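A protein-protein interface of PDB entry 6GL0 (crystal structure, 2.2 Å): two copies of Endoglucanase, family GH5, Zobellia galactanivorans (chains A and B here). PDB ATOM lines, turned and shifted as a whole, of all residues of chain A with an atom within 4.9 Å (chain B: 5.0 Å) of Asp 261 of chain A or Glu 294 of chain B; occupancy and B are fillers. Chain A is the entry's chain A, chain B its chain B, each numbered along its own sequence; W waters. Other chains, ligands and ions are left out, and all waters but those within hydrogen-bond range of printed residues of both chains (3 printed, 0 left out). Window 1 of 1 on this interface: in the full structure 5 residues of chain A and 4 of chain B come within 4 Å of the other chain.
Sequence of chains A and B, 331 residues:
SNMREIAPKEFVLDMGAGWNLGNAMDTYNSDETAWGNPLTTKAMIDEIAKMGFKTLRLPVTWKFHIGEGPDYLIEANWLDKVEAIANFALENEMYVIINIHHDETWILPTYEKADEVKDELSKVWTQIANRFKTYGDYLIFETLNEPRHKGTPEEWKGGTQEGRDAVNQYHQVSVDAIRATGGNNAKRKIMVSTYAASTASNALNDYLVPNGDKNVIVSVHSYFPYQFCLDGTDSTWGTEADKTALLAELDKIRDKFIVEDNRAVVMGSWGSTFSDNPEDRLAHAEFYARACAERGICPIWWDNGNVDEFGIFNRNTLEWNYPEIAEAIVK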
ATOM      1  N   LYS A 256     -17.427   0.282   5.788  1.00  0.00           N
ATOM      2  CA  LYS A 256     -17.347   1.714   5.986  1.00  0.00           C
ATOM      3  C   LYS A 256     -18.657   2.293   6.516  1.00  0.00           C
ATOM      4  O   LYS A 256     -18.647   2.900   7.564  1.00  0.00           O
ATOM      5  CB  LYS A 256     -16.884   2.413   4.698  1.00  0.00           C
ATOM      6  CG  LYS A 256     -17.176   3.912   4.566  1.00  0.00           C
ATOM      7  CD  LYS A 256     -16.410   4.761   5.546  1.00  0.00           C
ATOM      8  CE  LYS A 256     -16.927   6.191   5.450  1.00  0.00           C
ATOM      9  NZ  LYS A 256     -16.423   7.045   6.557  1.00  0.00           N
ATOM     10  N   PHE A 257     -19.775   2.118   5.817  1.00  0.00           N
ATOM     11  CA  PHE A 257     -20.967   2.867   6.184  1.00  0.00           C
ATOM     12  C   PHE A 257     -21.802   2.210   7.264  1.00  0.00           C
ATOM     13  O   PHE A 257     -22.329   2.904   8.155  1.00  0.00           O
ATOM     14  CB  PHE A 257     -21.849   3.155   4.983  1.00  0.00           C
ATOM     15  CG  PHE A 257     -21.241   4.116   4.009  1.00  0.00           C
ATOM     16  CD1 PHE A 257     -20.981   5.441   4.378  1.00  0.00           C
ATOM     17  CD2 PHE A 257     -20.900   3.716   2.720  1.00  0.00           C
ATOM     18  CE1 PHE A 257     -20.395   6.332   3.491  1.00  0.00           C
ATOM     19  CE2 PHE A 257     -20.329   4.613   1.830  1.00  0.00           C
ATOM     20  CZ  PHE A 257     -20.087   5.921   2.218  1.00  0.00           C
ATOM     21  N   ILE A 258     -21.948   0.884   7.177  1.00  0.00           N
ATOM     22  CA  ILE A 258     -22.867   0.172   8.049  1.00  0.00           C
ATOM     23  C   ILE A 258     -22.197  -0.150   9.387  1.00  0.00           C
ATOM     24  O   ILE A 258     -22.742   0.136  10.430  1.00  0.00           O
ATOM     25  CB  ILE A 258     -23.430  -1.088   7.353  1.00  0.00           C
ATOM     26  CG1 ILE A 258     -24.194  -0.657   6.102  1.00  0.00           C
ATOM     27  CG2 ILE A 258     -24.322  -1.895   8.304  1.00  0.00           C
ATOM     28  CD1 ILE A 258     -24.698  -1.768   5.214  1.00  0.00           C
ATOM     29  N   VAL A 259     -21.007  -0.727   9.343  1.00  0.00           N
ATOM     30  CA  VAL A 259     -20.341  -1.194  10.548  1.00  0.00           C
ATOM     31  C   VAL A 259     -19.678  -0.006  11.229  1.00  0.00           C
ATOM     32  O   VAL A 259     -20.058   0.352  12.328  1.00  0.00           O
ATOM     33  CB  VAL A 259     -19.318  -2.324  10.221  1.00  0.00           C
ATOM     34  CG1 VAL A 259     -18.506  -2.736  11.461  1.00  0.00           C
ATOM     35  CG2 VAL A 259     -20.056  -3.544   9.643  1.00  0.00           C
ATOM     36  N   GLU A 260     -18.696   0.597  10.574  1.00  0.00           N
ATOM     37  CA  GLU A 260     -17.907   1.653  11.194  1.00  0.00           C
ATOM     38  C   GLU A 260     -18.755   2.926  11.469  1.00  0.00           C
ATOM     39  O   GLU A 260     -18.633   3.505  12.512  1.00  0.00           O
ATOM     40  CB  GLU A 260     -16.651   1.921  10.381  1.00  0.00           C
ATOM     41  CG  GLU A 260     -15.852   3.142  10.814  1.00  0.00           C
ATOM     42  CD  GLU A 260     -14.538   3.308  10.084  1.00  0.00           C
ATOM     43  OE1 GLU A 260     -14.414   4.240   9.284  1.00  0.00           O
ATOM     44  OE2 GLU A 260     -13.581   2.547  10.349  1.00  0.00           O
ATOM     45  N   ASP A 261     -19.644   3.313  10.562  1.00  0.00           N
ATOM     46  CA  ASP A 261     -20.381   4.589  10.702  1.00  0.00           C
ATOM     47  C   ASP A 261     -21.804   4.426  11.221  1.00  0.00           C
ATOM     48  O   ASP A 261     -22.472   5.406  11.440  1.00  0.00           O
ATOM     49  CB  ASP A 261     -20.418   5.349   9.367  1.00  0.00           C
ATOM     50  CG  ASP A 261     -19.039   5.808   8.896  1.00  0.00           C
ATOM     51  OD1 ASP A 261     -18.031   5.663   9.618  1.00  0.00           O
ATOM     52  OD2 ASP A 261     -18.960   6.366   7.790  1.00  0.00           O
ATOM     53  N   ASN A 262     -22.279   3.196  11.412  1.00  0.00           N
ATOM     54  CA  ASN A 262     -23.679   2.938  11.828  1.00  0.00           C
ATOM     55  C   ASN A 262     -24.746   3.680  10.991  1.00  0.00           C
ATOM     56  O   ASN A 262     -25.711   4.254  11.507  1.00  0.00           O
ATOM     57  CB  ASN A 262     -23.863   3.160  13.350  1.00  0.00           C
ATOM     58  CG  ASN A 262     -25.167   2.584  13.870  1.00  0.00           C
ATOM     59  OD1 ASN A 262     -25.729   1.618  13.336  1.00  0.00           O
ATOM     60  ND2 ASN A 262     -25.695   3.221  14.885  1.00  0.00           N
ATOM     61  N   ARG A 263     -24.565   3.605   9.675  1.00  0.00           N
ATOM     62  CA  ARG A 263     -25.506   4.167   8.715  1.00  0.00           C
ATOM     63  C   ARG A 263     -26.189   3.080   7.889  1.00  0.00           C
ATOM     64  O   ARG A 263     -25.662   1.970   7.751  1.00  0.00           O
ATOM     65  CB  ARG A 263     -24.747   5.141   7.812  1.00  0.00           C
ATOM     66  CG  ARG A 263     -24.321   6.420   8.485  1.00  0.00           C
ATOM     67  CD  ARG A 263     -25.510   7.320   8.676  1.00  0.00           C
ATOM     68  NE  ARG A 263     -25.174   8.440   9.553  1.00  0.00           N
ATOM     69  CZ  ARG A 263     -26.040   9.376   9.940  1.00  0.00           C
ATOM     70  NH1 ARG A 263     -27.288   9.382   9.484  1.00  0.00           N
ATOM     71  NH2 ARG A 263     -25.640  10.317  10.768  1.00  0.00           N
ATOM     72  N   ARG B 254     -13.807  16.732  15.483  1.00  0.00           N
ATOM     73  CA  ARG B 254     -13.557  16.545  14.052  1.00  0.00           C
ATOM     74  C   ARG B 254     -13.716  17.843  13.234  1.00  0.00           C
ATOM     75  O   ARG B 254     -12.828  18.213  12.477  1.00  0.00           O
ATOM     76  CB  ARG B 254     -14.559  15.526  13.513  1.00  0.00           C
ATOM     77  CG  ARG B 254     -14.250  15.046  12.098  1.00  0.00           C
ATOM     78  CD  ARG B 254     -15.397  15.197  11.134  1.00  0.00           C
ATOM     79  NE  ARG B 254     -16.752  14.816  11.536  1.00  0.00           N
ATOM     80  CZ  ARG B 254     -17.342  13.649  11.257  1.00  0.00           C
ATOM     81  NH1 ARG B 254     -16.673  12.660  10.642  1.00  0.00           N
ATOM     82  NH2 ARG B 254     -18.625  13.451  11.621  1.00  0.00           N
ATOM     83  N   ARG B 290     -15.648   2.991  18.197  1.00  0.00           N
ATOM     84  CA  ARG B 290     -16.180   2.969  16.842  1.00  0.00           C
ATOM     85  C   ARG B 290     -16.345   4.408  16.279  1.00  0.00           C
ATOM     86  O   ARG B 290     -15.922   4.703  15.166  1.00  0.00           O
ATOM     87  CB  ARG B 290     -17.515   2.205  16.759  1.00  0.00           C
ATOM     88  CG  ARG B 290     -17.981   1.966  15.333  1.00  0.00           C
ATOM     89  CD  ARG B 290     -19.391   1.459  15.279  1.00  0.00           C
ATOM     90  NE  ARG B 290     -20.281   2.523  15.719  1.00  0.00           N
ATOM     91  CZ  ARG B 290     -21.416   2.332  16.385  1.00  0.00           C
ATOM     92  NH1 ARG B 290     -22.144   3.383  16.754  1.00  0.00           N
ATOM     93  NH2 ARG B 290     -21.843   1.114  16.705  1.00  0.00           N
ATOM     94  N   ALA B 291     -16.943   5.286  17.065  1.00  0.00           N
ATOM     95  CA  ALA B 291     -17.095   6.692  16.682  1.00  0.00           C
ATOM     96  C   ALA B 291     -15.771   7.420  16.415  1.00  0.00           C
ATOM     97  O   ALA B 291     -15.725   8.278  15.543  1.00  0.00           O
ATOM     98  CB  ALA B 291     -17.876   7.452  17.748  1.00  0.00           C
ATOM     99  N   CYS B 292     -14.718   7.092  17.179  1.00  0.00           N
ATOM    100  CA  CYS B 292     -13.372   7.593  16.939  1.00  0.00           C
ATOM    101  C   CYS B 292     -12.836   7.042  15.608  1.00  0.00           C
ATOM    102  O   CYS B 292     -12.334   7.809  14.772  1.00  0.00           O
ATOM    103  CB  CYS B 292     -12.423   7.223  18.073  1.00  0.00           C
ATOM    104  SG  CYS B 292     -12.600   8.234  19.580  1.00  0.00           S
ATOM    105  N   ALA B 293     -12.964   5.735  15.403  1.00  0.00           N
ATOM    106  CA  ALA B 293     -12.523   5.102  14.127  1.00  0.00           C
ATOM    107  C   ALA B 293     -13.204   5.744  12.910  1.00  0.00           C
ATOM    108  O   ALA B 293     -12.519   6.066  11.946  1.00  0.00           O
ATOM    109  CB  ALA B 293     -12.744   3.588  14.120  1.00  0.00           C
ATOM    110  N   GLU B 294     -14.520   5.969  12.994  1.00  0.00           N
ATOM    111  CA  GLU B 294     -15.290   6.639  11.945  1.00  0.00           C
ATOM    112  C   GLU B 294     -14.767   8.009  11.553  1.00  0.00           C
ATOM    113  O   GLU B 294     -14.862   8.399  10.382  1.00  0.00           O
ATOM    114  CB  GLU B 294     -16.747   6.866  12.378  1.00  0.00           C
ATOM    115  CG  GLU B 294     -17.526   7.899  11.543  1.00  0.00           C
ATOM    116  CD  GLU B 294     -19.024   8.012  11.881  1.00  0.00           C
ATOM    117  OE1 GLU B 294     -19.536   7.347  12.846  1.00  0.00           O
ATOM    118  OE2 GLU B 294     -19.707   8.800  11.169  1.00  0.00           O
ATOM    119  N   ARG B 295     -14.235   8.716  12.552  1.00  0.00           N
ATOM    120  CA  ARG B 295     -13.683  10.049  12.380  1.00  0.00           C
ATOM    121  C   ARG B 295     -12.171  10.070  12.174  1.00  0.00           C
ATOM    122  O   ARG B 295     -11.613  11.129  12.037  1.00  0.00           O
ATOM    123  CB  ARG B 295     -14.076  10.934  13.564  1.00  0.00           C
ATOM    124  CG  ARG B 295     -15.559  11.257  13.594  1.00  0.00           C
ATOM    125  CD  ARG B 295     -16.129  11.577  14.986  1.00  0.00           C
ATOM    126  NE  ARG B 295     -17.566  11.818  14.886  1.00  0.00           N
ATOM    127  CZ  ARG B 295     -18.491  10.879  14.692  1.00  0.00           C
ATOM    128  NH1 ARG B 295     -18.181   9.582  14.643  1.00  0.00           N
ATOM    129  NH2 ARG B 295     -19.773  11.228  14.561  1.00  0.00           N
ATOM    130  N   GLY B 296     -11.510   8.924  12.110  1.00  0.00           N
ATOM    131  CA  GLY B 296     -10.045   8.897  11.933  1.00  0.00           C
ATOM    132  C   GLY B 296      -9.246   9.305  13.165  1.00  0.00           C
ATOM    133  O   GLY B 296      -8.052   9.640  13.076  1.00  0.00           O
HETATM  134  O   HOH W   1     -22.437   8.297  10.760  1.00  0.00           O
HETATM  135  O   HOH W   2     -20.075   5.137  14.413  1.00  0.00           O
HETATM  136  O   HOH W   3     -24.158   5.875  15.893  1.00  0.00           O
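No position is printed for both chains. Of the 6 pairs that touch across the chains among the printed residues, none has its exchanged pair printed and touching as well.
Among the printed residues, merely in contact across the chains: Asp 261 of chain A with Glu 294 of chain B, Val 259 of chain A with Arg 290 of chain B, Glu 260 of chain A with Arg 290 of chain B, Glu 260 of chain A with Glu 294 of chain B, Glu 260 of chain A with Ala 293 of chain B and Asn 262 of chain A with Arg 290 of chain B.
The side-chain amino group of Lys 256 of chain A lies within salt-bridge range of the side-chain carboxylate of Asp 261 of chain A, at 2.9 Å. O of Phe 257 of chain A is in hydrogen-bond range of N of Asn 262 of chain A (3.3 Å). The side-chain carboxylate of Glu 294 of chain B is in salt-bridge range of the guanidinium group of Arg 295 of chain B, at 3.2 Å.
Asp 261 of chain A touches just one residue of chain B: Glu 294 (3.0 Å). Of the printed residues of chain A, Glu 294 of chain B touches Glu 260 (3.7 Å) and Asp 261 (3.0 Å). Of the printed residues of chain A, Ala 293 of chain B touches Glu 260 (3.7 Å). Printed residues of chain B within 4 Å of Glu 260 of chain A: Arg 290, Ala 293 and Glu 294. Of the printed residues of chain B, Asn 262 of chain A touches Arg 290.
Water W2 lies within hydrogen-bond range of OE1 of Glu 294 of chain B, O of Glu 260 of chain A and NE of Arg 290 of chain B. Water W1 lies within hydrogen-bond range of the side-chain carboxylate of Glu 294 of chain B (2.8 Å), the backbone carbonyl oxygen of Asp 261 of chain A (3.0 Å) and the guanidinium group of Arg 263 of chain A (3.0 Å). Water W3 lies within hydrogen-bond range of the side-chain amide nitrogen of Asn 262 of chain A (3.2 Å) and the guanidinium group of Arg 290 of chain B (3.3 Å).
Of the 8 printed residues of chain A, 4 touch a printed residue of chain B. Printed residues of chain A that touch a printed residue of chain B: Val 259, Glu 260, Asp 261 and Asn 262. Printed residues of chain B that touch a printed residue of chain A: Arg 290, Ala 293 and Glu 294. Among the printed residues, no Asp or Glu carboxylate lies within 4 Å of a Lys or Arg side-chain nitrogen of the other chain.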
